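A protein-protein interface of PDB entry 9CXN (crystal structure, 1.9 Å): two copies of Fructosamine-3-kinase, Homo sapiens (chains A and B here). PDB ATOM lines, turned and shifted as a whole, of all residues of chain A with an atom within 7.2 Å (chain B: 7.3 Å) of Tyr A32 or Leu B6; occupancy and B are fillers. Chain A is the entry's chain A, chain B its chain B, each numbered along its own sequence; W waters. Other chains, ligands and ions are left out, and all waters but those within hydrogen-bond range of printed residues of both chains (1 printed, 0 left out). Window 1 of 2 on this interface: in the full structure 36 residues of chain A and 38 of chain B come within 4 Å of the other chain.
Leu B6 touches Tyr A32. Arg B16 touches Tyr A32. Phe B18 touches Tyr A32 (CE1 to C, 3.9 Å). O of Thr B14 touches O of Asp A33 (3.8 Å). Asp A33 touches Leu B15. Thr A34 touches Thr B14. Thr A34 touches Leu B15 (CG2 to CD1, 3.997 Å). CD2 of Leu B5 touches CG2 of Ile A78, at 3.8 Å. CG2 of Val A88 touches CD2 of Leu B6, at 3.9 Å. NE2 of His A91 touches CE2 of Phe B18, 3.5 Å away.
No position is printed for both chains. Of the 18 pairs that touch across the chains among the printed residues, none has its exchanged pair printed and touching as well.
Of the printed residues of chain B, Tyr A32 touches Leu B6, Leu B15, Arg B16, Ala B17 and Phe B18. Printed residues of chain A within 4 Å of Leu B6: Tyr A32 (3.8 Å) and Val A88 (3.9 Å). Printed residues of chain A within 4 Å of Thr B12: Thr A34 (3.6 Å). Of the printed residues of chain A, Arg B16 touches Tyr A32 and Asp A33. Of the printed residues of chain A, Thr B14 touches Asp A33 (3.8 Å) and Thr A34 (3.7 Å). Printed residues of chain B within 4 Å of Val A88: Leu B6 (3.9 Å). Printed residues of chain A within 4 Å of Leu B5: Ile A78. The nearest printed residue of chain B that does not touch Ala A31 is Arg B16 (4.4 Å).
The backbone carbonyl oxygen (O) of Val A39 sits at hydrogen-bond distance from the backbone NH (N) of Tyr A32. The backbone carbonyl oxygen (O) of Gly A37 is in hydrogen-bond range of the side-chain hydroxyl (OG1) of Thr A34. O of Pro A38 lies within hydrogen-bond range of N of His A91 (3.2 Å). The backbone NH of Ile A78 sits at hydrogen-bond distance from the backbone carbonyl oxygen of Ala A86, 2.8 Å away. O of Arg B7 lies within hydrogen-bond range of N of Thr B12. O of Thr B14 is in hydrogen-bond range of OG1 of Thr B12 (2.6 Å).
O of Ala A31 is in hydrogen-bond range of N of Phe B18, at 2.9 Å. The backbone NH of Asp A33 lies within hydrogen-bond range of the backbone carbonyl oxygen of Arg B16.
Water W1 lies within hydrogen-bond range of the side-chain carboxylate (OE2) of Glu B3 (2.5 Å) and the side-chain hydroxyl (OH) of Tyr A32 (2.8 Å).
Printed residues of chain A that touch a printed residue of chain B: Ala A31, Tyr A32, Asp A33, Thr A34, Ile A78, Val A88 and His A91. Hydrophobic or aromatic side chains of chain A within 4 Å of the printed part of chain B: Ala A31, Tyr A32, Ile A78, Val A88 and His A91. Of the 19 printed residues of chain B, 9 touch a printed residue of chain A. Along chain B the printed residues that touch a printed residue of chain A span positions 5 to 18. Among the printed residues, 18 pairs touch across the chains. Among the printed residues, no Asp or Glu carboxylate lies within 4 Å of a Lys or Arg side-chain nitrogen of the other chain.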
ATOM      1  N   GLY A  29      -0.146  -3.603   0.689  1.00  0.00           N
ATOM      2  CA  GLY A  29       0.098  -2.324   0.035  1.00  0.00           C
ATOM      3  C   GLY A  29       1.546  -1.903   0.189  1.00  0.00           C
ATOM      4  O   GLY A  29       2.411  -2.730   0.445  1.00  0.00           O
ATOM      5  N   ARG A  30       1.797  -0.601   0.013  1.00  0.00           N
ATOM      6  CA  ARG A  30       3.150  -0.061   0.056  1.00  0.00           C
ATOM      7  C   ARG A  30       3.152   1.346   0.631  1.00  0.00           C
ATOM      8  O   ARG A  30       2.273   2.142   0.319  1.00  0.00           O
ATOM      9  CB  ARG A  30       3.812  -0.016  -1.350  1.00  0.00           C
ATOM     10  N   ALA A  31       4.180   1.665   1.414  1.00  0.00           N
ATOM     11  CA  ALA A  31       4.448   2.972   2.002  1.00  0.00           C
ATOM     12  C   ALA A  31       5.440   3.761   1.166  1.00  0.00           C
ATOM     13  O   ALA A  31       6.396   3.198   0.625  1.00  0.00           O
ATOM     14  CB  ALA A  31       5.039   2.831   3.396  1.00  0.00           C
ATOM     15  N   TYR A  32       5.243   5.084   1.122  1.00  0.00           N
ATOM     16  CA  TYR A  32       6.072   6.001   0.344  1.00  0.00           C
ATOM     17  C   TYR A  32       6.348   7.244   1.153  1.00  0.00           C
ATOM     18  O   TYR A  32       5.433   7.790   1.759  1.00  0.00           O
ATOM     19  CB  TYR A  32       5.397   6.480  -0.984  1.00  0.00           C
ATOM     20  CG  TYR A  32       5.047   5.377  -1.966  1.00  0.00           C
ATOM     21  CD1 TYR A  32       3.879   4.647  -1.829  1.00  0.00           C
ATOM     22  CD2 TYR A  32       5.886   5.076  -3.061  1.00  0.00           C
ATOM     23  CE1 TYR A  32       3.547   3.633  -2.706  1.00  0.00           C
ATOM     24  CE2 TYR A  32       5.543   4.073  -3.949  1.00  0.00           C
ATOM     25  CZ  TYR A  32       4.393   3.363  -3.786  1.00  0.00           C
ATOM     26  OH  TYR A  32       4.047   2.342  -4.649  1.00  0.00           O
ATOM     27  N   ASP A  33       7.577   7.753   1.062  1.00  0.00           N
ATOM     28  CA  ASP A  33       7.884   9.101   1.527  1.00  0.00           C
ATOM     29  C   ASP A  33       7.460  10.123   0.469  1.00  0.00           C
ATOM     30  O   ASP A  33       7.600   9.883  -0.728  1.00  0.00           O
ATOM     31  CB  ASP A  33       9.391   9.216   1.810  1.00  0.00           C
ATOM     32  CG  ASP A  33       9.815   8.504   3.122  1.00  0.00           C
ATOM     33  OD1 ASP A  33       8.998   8.379   4.071  1.00  0.00           O
ATOM     34  OD2 ASP A  33      10.971   8.036   3.187  1.00  0.00           O
ATOM     35  N   THR A  34       6.856  11.232   0.903  1.00  0.00           N
ATOM     36  CA  THR A  34       6.410  12.278  -0.015  1.00  0.00           C
ATOM     37  C   THR A  34       6.781  13.627   0.559  1.00  0.00           C
ATOM     38  O   THR A  34       7.349  13.731   1.652  1.00  0.00           O
ATOM     39  CB  THR A  34       4.891  12.280  -0.296  1.00  0.00           C
ATOM     40  OG1 THR A  34       4.214  13.149   0.647  1.00  0.00           O
ATOM     41  CG2 THR A  34       4.320  10.896  -0.256  1.00  0.00           C
ATOM     42  N   GLY A  37       5.015  14.391   3.838  1.00  0.00           N
ATOM     43  CA  GLY A  37       5.149  13.355   4.825  1.00  0.00           C
ATOM     44  C   GLY A  37       4.830  11.984   4.268  1.00  0.00           C
ATOM     45  O   GLY A  37       4.513  11.819   3.083  1.00  0.00           O
ATOM     46  N   PRO A  38       4.891  10.970   5.115  1.00  0.00           N
ATOM     47  CA  PRO A  38       4.777   9.597   4.617  1.00  0.00           C
ATOM     48  C   PRO A  38       3.329   9.242   4.331  1.00  0.00           C
ATOM     49  O   PRO A  38       2.412   9.750   4.981  1.00  0.00           O
ATOM     50  CB  PRO A  38       5.350   8.762   5.770  1.00  0.00           C
ATOM     51  CG  PRO A  38       6.053   9.749   6.649  1.00  0.00           C
ATOM     52  CD  PRO A  38       5.283  11.004   6.527  1.00  0.00           C
ATOM     53  N   VAL A  39       3.122   8.339   3.351  1.00  0.00           N
ATOM     54  CA  VAL A  39       1.783   7.853   3.043  1.00  0.00           C
ATOM     55  C   VAL A  39       1.842   6.353   2.881  1.00  0.00           C
ATOM     56  O   VAL A  39       2.890   5.762   2.562  1.00  0.00           O
ATOM     57  CB  VAL A  39       1.180   8.504   1.755  1.00  0.00           C
ATOM     58  CG1 VAL A  39       1.160  10.006   1.875  1.00  0.00           C
ATOM     59  CG2 VAL A  39       1.987   8.057   0.471  1.00  0.00           C
ATOM     60  N   PHE A  40       0.683   5.735   3.045  1.00  0.00           N
ATOM     61  CA  PHE A  40       0.512   4.323   2.786  1.00  0.00           C
ATOM     62  C   PHE A  40      -0.546   4.140   1.700  1.00  0.00           C
ATOM     63  O   PHE A  40      -1.606   4.777   1.742  1.00  0.00           O
ATOM     64  CB  PHE A  40       0.127   3.558   4.098  1.00  0.00           C
ATOM     65  CG  PHE A  40       0.126   2.068   3.927  1.00  0.00           C
ATOM     66  CD1 PHE A  40       1.302   1.335   4.070  1.00  0.00           C
ATOM     67  CD2 PHE A  40      -1.019   1.398   3.595  1.00  0.00           C
ATOM     68  CE1 PHE A  40       1.307  -0.042   3.887  1.00  0.00           C
ATOM     69  CE2 PHE A  40      -1.013   0.019   3.411  1.00  0.00           C
ATOM     70  CZ  PHE A  40       0.167  -0.697   3.564  1.00  0.00           C
ATOM     71  N   VAL A  41      -0.293   3.249   0.744  1.00  0.00           N
ATOM     72  CA  VAL A  41      -1.114   3.096  -0.453  1.00  0.00           C
ATOM     73  C   VAL A  41      -1.552   1.652  -0.587  1.00  0.00           C
ATOM     74  O   VAL A  41      -0.715   0.743  -0.756  1.00  0.00           O
ATOM     75  CB  VAL A  41      -0.341   3.548  -1.734  1.00  0.00           C
ATOM     76  CG1 VAL A  41      -1.205   3.348  -2.934  1.00  0.00           C
ATOM     77  CG2 VAL A  41       0.038   5.011  -1.611  1.00  0.00           C
ATOM     78  N   LYS A  42      -2.851   1.437  -0.610  1.00  0.00           N
ATOM     79  CA  LYS A  42      -3.395   0.133  -0.928  1.00  0.00           C
ATOM     80  C   LYS A  42      -3.856   0.109  -2.372  1.00  0.00           C
ATOM     81  O   LYS A  42      -4.472   1.066  -2.853  1.00  0.00           O
ATOM     82  CB  LYS A  42      -4.592  -0.215  -0.008  1.00  0.00           C
ATOM     83  CG  LYS A  42      -4.276  -0.371   1.440  1.00  0.00           C
ATOM     84  CD  LYS A  42      -5.594  -0.757   2.193  1.00  0.00           C
ATOM     85  CE  LYS A  42      -5.399  -0.828   3.689  1.00  0.00           C
ATOM     86  NZ  LYS A  42      -6.616  -1.347   4.421  1.00  0.00           N
ATOM     87  N   VAL A  43      -3.644  -1.021  -3.048  1.00  0.00           N
ATOM     88  CA  VAL A  43      -4.006  -1.152  -4.451  1.00  0.00           C
ATOM     89  C   VAL A  43      -4.862  -2.399  -4.628  1.00  0.00           C
ATOM     90  O   VAL A  43      -4.559  -3.448  -4.058  1.00  0.00           O
ATOM     91  CB  VAL A  43      -2.731  -1.226  -5.336  1.00  0.00           C
ATOM     92  CG1 VAL A  43      -3.123  -1.471  -6.762  1.00  0.00           C
ATOM     93  CG2 VAL A  43      -1.881   0.034  -5.157  1.00  0.00           C
ATOM     94  N   ILE A  78      -8.302   6.710  -5.686  1.00  0.00           N
ATOM     95  CA  ILE A  78      -7.938   6.990  -7.081  1.00  0.00           C
ATOM     96  C   ILE A  78      -8.370   5.831  -7.958  1.00  0.00           C
ATOM     97  O   ILE A  78      -7.986   4.683  -7.695  1.00  0.00           O
ATOM     98  CB  ILE A  78      -6.420   7.192  -7.251  1.00  0.00           C
ATOM     99  CG1 ILE A  78      -5.903   8.258  -6.295  1.00  0.00           C
ATOM    100  CG2 ILE A  78      -6.093   7.471  -8.732  1.00  0.00           C
ATOM    101  CD1 ILE A  78      -4.476   8.145  -5.986  1.00  0.00           C
ATOM    102  N   ALA A  86      -6.655   2.679  -6.097  1.00  0.00           N
ATOM    103  CA  ALA A  86      -5.707   2.838  -5.018  1.00  0.00           C
ATOM    104  C   ALA A  86      -6.348   3.692  -3.937  1.00  0.00           C
ATOM    105  O   ALA A  86      -7.182   4.548  -4.236  1.00  0.00           O
ATOM    106  CB  ALA A  86      -4.422   3.542  -5.432  1.00  0.00           C
ATOM    107  N   PHE A  87      -5.945   3.461  -2.687  1.00  0.00           N
ATOM    108  CA  PHE A  87      -6.447   4.218  -1.539  1.00  0.00           C
ATOM    109  C   PHE A  87      -5.241   4.710  -0.782  1.00  0.00           C
ATOM    110  O   PHE A  87      -4.404   3.903  -0.371  1.00  0.00           O
ATOM    111  CB  PHE A  87      -7.393   3.346  -0.659  1.00  0.00           C
ATOM    112  CG  PHE A  87      -7.746   3.972   0.666  1.00  0.00           C
ATOM    113  CD1 PHE A  87      -7.898   5.351   0.812  1.00  0.00           C
ATOM    114  CD2 PHE A  87      -7.950   3.155   1.788  1.00  0.00           C
ATOM    115  CE1 PHE A  87      -8.235   5.925   2.063  1.00  0.00           C
ATOM    116  CE2 PHE A  87      -8.286   3.697   3.023  1.00  0.00           C
ATOM    117  CZ  PHE A  87      -8.429   5.097   3.171  1.00  0.00           C
ATOM    118  N   VAL A  88      -5.098   6.023  -0.685  1.00  0.00           N
ATOM    119  CA  VAL A  88      -3.975   6.659  -0.027  1.00  0.00           C
ATOM    120  C   VAL A  88      -4.427   7.136   1.340  1.00  0.00           C
ATOM    121  O   VAL A  88      -5.451   7.839   1.454  1.00  0.00           O
ATOM    122  CB  VAL A  88      -3.427   7.860  -0.833  1.00  0.00           C
ATOM    123  CG1 VAL A  88      -2.198   8.421  -0.166  1.00  0.00           C
ATOM    124  CG2 VAL A  88      -3.154   7.471  -2.287  1.00  0.00           C
ATOM    125  N   HIS A  91       0.528   7.811   6.684  1.00  0.00           N
ATOM    126  CA  HIS A  91       1.390   6.782   7.217  1.00  0.00           C
ATOM    127  C   HIS A  91       1.683   7.061   8.684  1.00  0.00           C
ATOM    128  O   HIS A  91       1.920   8.197   9.074  1.00  0.00           O
ATOM    129  CB  HIS A  91       2.694   6.696   6.417  1.00  0.00           C
ATOM    130  CG  HIS A  91       3.754   5.893   7.092  1.00  0.00           C
ATOM    131  ND1 HIS A  91       4.621   6.441   8.021  1.00  0.00           N
ATOM    132  CD2 HIS A  91       4.112   4.593   6.956  1.00  0.00           C
ATOM    133  CE1 HIS A  91       5.457   5.505   8.439  1.00  0.00           C
ATOM    134  NE2 HIS A  91       5.178   4.378   7.802  1.00  0.00           N
ATOM    135  N   ALA B   1       3.122   4.796 -14.758  1.00  0.00           N
ATOM    136  CA  ALA B   1       2.562   3.728 -13.935  1.00  0.00           C
ATOM    137  C   ALA B   1       2.147   4.281 -12.557  1.00  0.00           C
ATOM    138  O   ALA B   1       1.873   5.479 -12.427  1.00  0.00           O
ATOM    139  CB  ALA B   1       3.546   2.588 -13.799  1.00  0.00           C
ATOM    140  N   MET B   2       2.111   3.414 -11.543  1.00  0.00           N
ATOM    141  CA  MET B   2       1.466   3.780 -10.285  1.00  0.00           C
ATOM    142  C   MET B   2       2.162   4.968  -9.631  1.00  0.00           C
ATOM    143  O   MET B   2       1.515   5.864  -9.077  1.00  0.00           O
ATOM    144  CB  MET B   2       1.480   2.576  -9.337  1.00  0.00           C
ATOM    145  CG  MET B   2       0.112   1.929  -9.236  1.00  0.00           C
ATOM    146  SD  MET B   2      -1.109   2.864  -8.334  1.00  0.00           S
ATOM    147  CE  MET B   2      -0.020   3.623  -7.124  1.00  0.00           C
ATOM    148  N   GLU B   3       3.480   5.006  -9.713  1.00  0.00           N
ATOM    149  CA  GLU B   3       4.231   6.050  -9.039  1.00  0.00           C
ATOM    150  C   GLU B   3       4.030   7.414  -9.687  1.00  0.00           C
ATOM    151  O   GLU B   3       3.932   8.421  -8.989  1.00  0.00           O
ATOM    152  CB  GLU B   3       5.690   5.643  -9.005  1.00  0.00           C
ATOM    153  CG  GLU B   3       5.852   4.341  -8.234  1.00  0.00           C
ATOM    154  CD  GLU B   3       7.258   4.137  -7.672  1.00  0.00           C
ATOM    155  OE1 GLU B   3       8.047   5.124  -7.561  1.00  0.00           O
ATOM    156  OE2 GLU B   3       7.552   2.968  -7.327  1.00  0.00           O
ATOM    157  N   GLN B   4       3.926   7.474 -11.025  1.00  0.00           N
ATOM    158  CA  GLN B   4       3.623   8.761 -11.647  1.00  0.00           C
ATOM    159  C   GLN B   4       2.211   9.224 -11.279  1.00  0.00           C
ATOM    160  O   GLN B   4       1.978  10.405 -11.023  1.00  0.00           O
ATOM    161  CB  GLN B   4       3.815   8.650 -13.157  1.00  0.00           C
ATOM    162  CG  GLN B   4       5.305   8.396 -13.513  1.00  0.00           C
ATOM    163  CD  GLN B   4       6.186   9.544 -13.034  1.00  0.00           C
ATOM    164  OE1 GLN B   4       5.761  10.695 -13.066  1.00  0.00           O
ATOM    165  NE2 GLN B   4       7.417   9.249 -12.625  1.00  0.00           N
ATOM    166  N   LEU B   5       1.274   8.281 -11.206  1.00  0.00           N
ATOM    167  CA  LEU B   5      -0.080   8.639 -10.809  1.00  0.00           C
ATOM    168  C   LEU B   5      -0.105   9.215  -9.398  1.00  0.00           C
ATOM    169  O   LEU B   5      -0.746  10.244  -9.159  1.00  0.00           O
ATOM    170  CB  LEU B   5      -0.981   7.420 -10.912  1.00  0.00           C
ATOM    171  CG  LEU B   5      -2.466   7.725 -10.860  1.00  0.00           C
ATOM    172  CD1 LEU B   5      -2.884   8.728 -11.960  1.00  0.00           C
ATOM    173  CD2 LEU B   5      -3.203   6.409 -11.016  1.00  0.00           C
ATOM    174  N   LEU B   6       0.637   8.596  -8.474  1.00  0.00           N
ATOM    175  CA  LEU B   6       0.696   9.076  -7.094  1.00  0.00           C
ATOM    176  C   LEU B   6       1.307  10.452  -7.034  1.00  0.00           C
ATOM    177  O   LEU B   6       0.791  11.337  -6.342  1.00  0.00           O
ATOM    178  CB  LEU B   6       1.501   8.120  -6.215  1.00  0.00           C
ATOM    179  CG  LEU B   6       0.793   6.793  -5.922  1.00  0.00           C
ATOM    180  CD1 LEU B   6       1.703   5.799  -5.172  1.00  0.00           C
ATOM    181  CD2 LEU B   6      -0.485   7.077  -5.093  1.00  0.00           C
ATOM    182  N   ARG B   7       2.433  10.661  -7.754  1.00  0.00           N
ATOM    183  CA  ARG B   7       3.031  11.987  -7.727  1.00  0.00           C
ATOM    184  C   ARG B   7       2.038  13.040  -8.189  1.00  0.00           C
ATOM    185  O   ARG B   7       1.989  14.150  -7.636  1.00  0.00           O
ATOM    186  CB  ARG B   7       4.310  12.064  -8.603  1.00  0.00           C
ATOM    187  CG  ARG B   7       5.464  11.254  -8.125  1.00  0.00           C
ATOM    188  CD  ARG B   7       6.573  11.152  -9.222  1.00  0.00           C
ATOM    189  NE  ARG B   7       7.653  10.242  -8.841  1.00  0.00           N
ATOM    190  CZ  ARG B   7       8.798  10.610  -8.278  1.00  0.00           C
ATOM    191  NH1 ARG B   7       9.043  11.876  -7.969  1.00  0.00           N
ATOM    192  NH2 ARG B   7       9.704   9.675  -7.979  1.00  0.00           N
ATOM    193  N   ALA B   8       1.258  12.726  -9.234  1.00  0.00           N
ATOM    194  CA  ALA B   8       0.293  13.700  -9.749  1.00  0.00           C
ATOM    195  C   ALA B   8      -0.880  13.908  -8.804  1.00  0.00           C
ATOM    196  O   ALA B   8      -1.348  15.030  -8.614  1.00  0.00           O
ATOM    197  CB  ALA B   8      -0.236  13.222 -11.100  1.00  0.00           C
ATOM    198  N   GLU B   9      -1.471  12.814  -8.325  1.00  0.00           N
ATOM    199  CA  GLU B   9      -2.653  12.913  -7.479  1.00  0.00           C
ATOM    200  C   GLU B   9      -2.337  13.602  -6.154  1.00  0.00           C
ATOM    201  O   GLU B   9      -3.169  14.349  -5.625  1.00  0.00           O
ATOM    202  CB  GLU B   9      -3.210  11.512  -7.243  1.00  0.00           C
ATOM    203  CG  GLU B   9      -3.766  10.863  -8.490  1.00  0.00           C
ATOM    204  CD  GLU B   9      -5.195  11.297  -8.776  1.00  0.00           C
ATOM    205  OE1 GLU B   9      -5.806  11.950  -7.891  1.00  0.00           O
ATOM    206  OE2 GLU B   9      -5.706  10.942  -9.862  1.00  0.00           O
ATOM    207  N   LEU B  10      -1.152  13.348  -5.602  1.00  0.00           N
ATOM    208  CA  LEU B  10      -0.737  13.919  -4.329  1.00  0.00           C
ATOM    209  C   LEU B  10       0.022  15.221  -4.489  1.00  0.00           C
ATOM    210  O   LEU B  10       0.319  15.864  -3.479  1.00  0.00           O
ATOM    211  CB  LEU B  10       0.145  12.929  -3.538  1.00  0.00           C
ATOM    212  CG  LEU B  10      -0.504  11.585  -3.222  1.00  0.00           C
ATOM    213  CD1 LEU B  10       0.413  10.623  -2.450  1.00  0.00           C
ATOM    214  CD2 LEU B  10      -1.844  11.798  -2.490  1.00  0.00           C
ATOM    215  N   ARG B  11       0.380  15.601  -5.722  1.00  0.00           N
ATOM    216  CA  ARG B  11       1.065  16.866  -5.976  1.00  0.00           C
ATOM    217  C   ARG B  11       2.347  16.950  -5.168  1.00  0.00           C
ATOM    218  O   ARG B  11       2.614  17.940  -4.499  1.00  0.00           O
ATOM    219  CB  ARG B  11       0.145  18.049  -5.659  1.00  0.00           C
ATOM    220  CG  ARG B  11      -1.182  18.010  -6.394  1.00  0.00           C
ATOM    221  N   THR B  12       3.180  15.934  -5.299  1.00  0.00           N
ATOM    222  CA  THR B  12       4.441  15.820  -4.574  1.00  0.00           C
ATOM    223  C   THR B  12       5.587  15.655  -5.562  1.00  0.00           C
ATOM    224  O   THR B  12       5.460  14.935  -6.558  1.00  0.00           O
ATOM    225  CB  THR B  12       4.409  14.612  -3.594  1.00  0.00           C
ATOM    226  OG1 THR B  12       5.717  14.383  -3.044  1.00  0.00           O
ATOM    227  CG2 THR B  12       3.937  13.340  -4.297  1.00  0.00           C
ATOM    228  N   THR B  14       8.729  14.435  -4.579  1.00  0.00           N
ATOM    229  CA  THR B  14       9.387  13.184  -4.212  1.00  0.00           C
ATOM    230  C   THR B  14       8.377  12.070  -3.969  1.00  0.00           C
ATOM    231  O   THR B  14       7.212  12.301  -3.636  1.00  0.00           O
ATOM    232  CB  THR B  14      10.252  13.342  -2.967  1.00  0.00           C
ATOM    233  OG1 THR B  14       9.492  14.030  -1.968  1.00  0.00           O
ATOM    234  CG2 THR B  14      11.493  14.149  -3.310  1.00  0.00           C
ATOM    235  N   LEU B  15       8.836  10.852  -4.175  1.00  0.00           N
ATOM    236  CA  LEU B  15       8.013   9.701  -3.894  1.00  0.00           C
ATOM    237  C   LEU B  15       8.876   8.453  -3.766  1.00  0.00           C
ATOM    238  O   LEU B  15       9.016   7.695  -4.734  1.00  0.00           O
ATOM    239  CB  LEU B  15       6.952   9.518  -4.980  1.00  0.00           C
ATOM    240  CG  LEU B  15       5.898   8.515  -4.544  1.00  0.00           C
ATOM    241  CD1 LEU B  15       4.727   9.209  -3.857  1.00  0.00           C
ATOM    242  CD2 LEU B  15       5.427   7.621  -5.688  1.00  0.00           C
ATOM    243  N   ARG B  16       9.489   8.243  -2.607  1.00  0.00           N
ATOM    244  CA  ARG B  16      10.427   7.147  -2.430  1.00  0.00           C
ATOM    245  C   ARG B  16       9.768   6.003  -1.666  1.00  0.00           C
ATOM    246  O   ARG B  16       9.394   6.173  -0.498  1.00  0.00           O
ATOM    247  CB  ARG B  16      11.673   7.621  -1.697  1.00  0.00           C
ATOM    248  CG  ARG B  16      12.748   6.555  -1.717  1.00  0.00           C
ATOM    249  CD  ARG B  16      13.218   6.331  -3.148  1.00  0.00           C
ATOM    250  NE  ARG B  16      14.345   5.408  -3.166  1.00  0.00           N
ATOM    251  CZ  ARG B  16      15.619   5.771  -3.247  1.00  0.00           C
ATOM    252  NH1 ARG B  16      16.579   4.873  -3.179  1.00  0.00           N
ATOM    253  NH2 ARG B  16      15.935   7.070  -3.383  1.00  0.00           N
ATOM    254  N   ALA B  17       9.617   4.848  -2.322  1.00  0.00           N
ATOM    255  CA  ALA B  17       9.045   3.677  -1.663  1.00  0.00           C
ATOM    256  C   ALA B  17       9.904   3.214  -0.481  1.00  0.00           C
ATOM    257  O   ALA B  17      11.128   3.406  -0.453  1.00  0.00           O
ATOM    258  CB  ALA B  17       8.866   2.517  -2.654  1.00  0.00           C
ATOM    259  N   PHE B  18       9.244   2.624   0.519  1.00  0.00           N
ATOM    260  CA  PHE B  18       9.971   1.983   1.608  1.00  0.00           C
ATOM    261  C   PHE B  18      10.626   0.697   1.090  1.00  0.00           C
ATOM    262  O   PHE B  18      10.077   0.002   0.221  1.00  0.00           O
ATOM    263  CB  PHE B  18       9.020   1.641   2.752  1.00  0.00           C
ATOM    264  CG  PHE B  18       8.670   2.807   3.637  1.00  0.00           C
ATOM    265  CD1 PHE B  18       8.541   4.099   3.113  1.00  0.00           C
ATOM    266  CD2 PHE B  18       8.370   2.602   4.986  1.00  0.00           C
ATOM    267  CE1 PHE B  18       8.171   5.171   3.934  1.00  0.00           C
ATOM    268  CE2 PHE B  18       7.986   3.681   5.824  1.00  0.00           C
ATOM    269  CZ  PHE B  18       7.884   4.955   5.298  1.00  0.00           C
ATOM    270  N   PHE B 234       3.756  -6.599 -10.457  1.00  0.00           N
ATOM    271  CA  PHE B 234       3.464  -5.772  -9.287  1.00  0.00           C
ATOM    272  C   PHE B 234       4.178  -4.417  -9.337  1.00  0.00           C
ATOM    273  O   PHE B 234       4.021  -3.621  -8.415  1.00  0.00           O
ATOM    274  CB  PHE B 234       3.809  -6.526  -8.017  1.00  0.00           C
ATOM    275  CG  PHE B 234       2.971  -7.763  -7.816  1.00  0.00           C
ATOM    276  CD1 PHE B 234       1.606  -7.673  -7.668  1.00  0.00           C
ATOM    277  CD2 PHE B 234       3.551  -9.015  -7.793  1.00  0.00           C
ATOM    278  CE1 PHE B 234       0.834  -8.821  -7.462  1.00  0.00           C
ATOM    279  CE2 PHE B 234       2.819 -10.148  -7.594  1.00  0.00           C
ATOM    280  CZ  PHE B 234       1.434 -10.061  -7.428  1.00  0.00           C
ATOM    281  N   GLY B 236       7.091  -1.254  -9.686  1.00  0.00           N
ATOM    282  CA  GLY B 236       8.139  -0.862  -8.772  1.00  0.00           C
ATOM    283  C   GLY B 236       9.550  -0.874  -9.340  1.00  0.00           C
ATOM    284  O   GLY B 236      10.475  -0.393  -8.663  1.00  0.00           O
HETATM  285  O   HOH W   1       5.720   1.387  -6.733  1.00  0.00           O
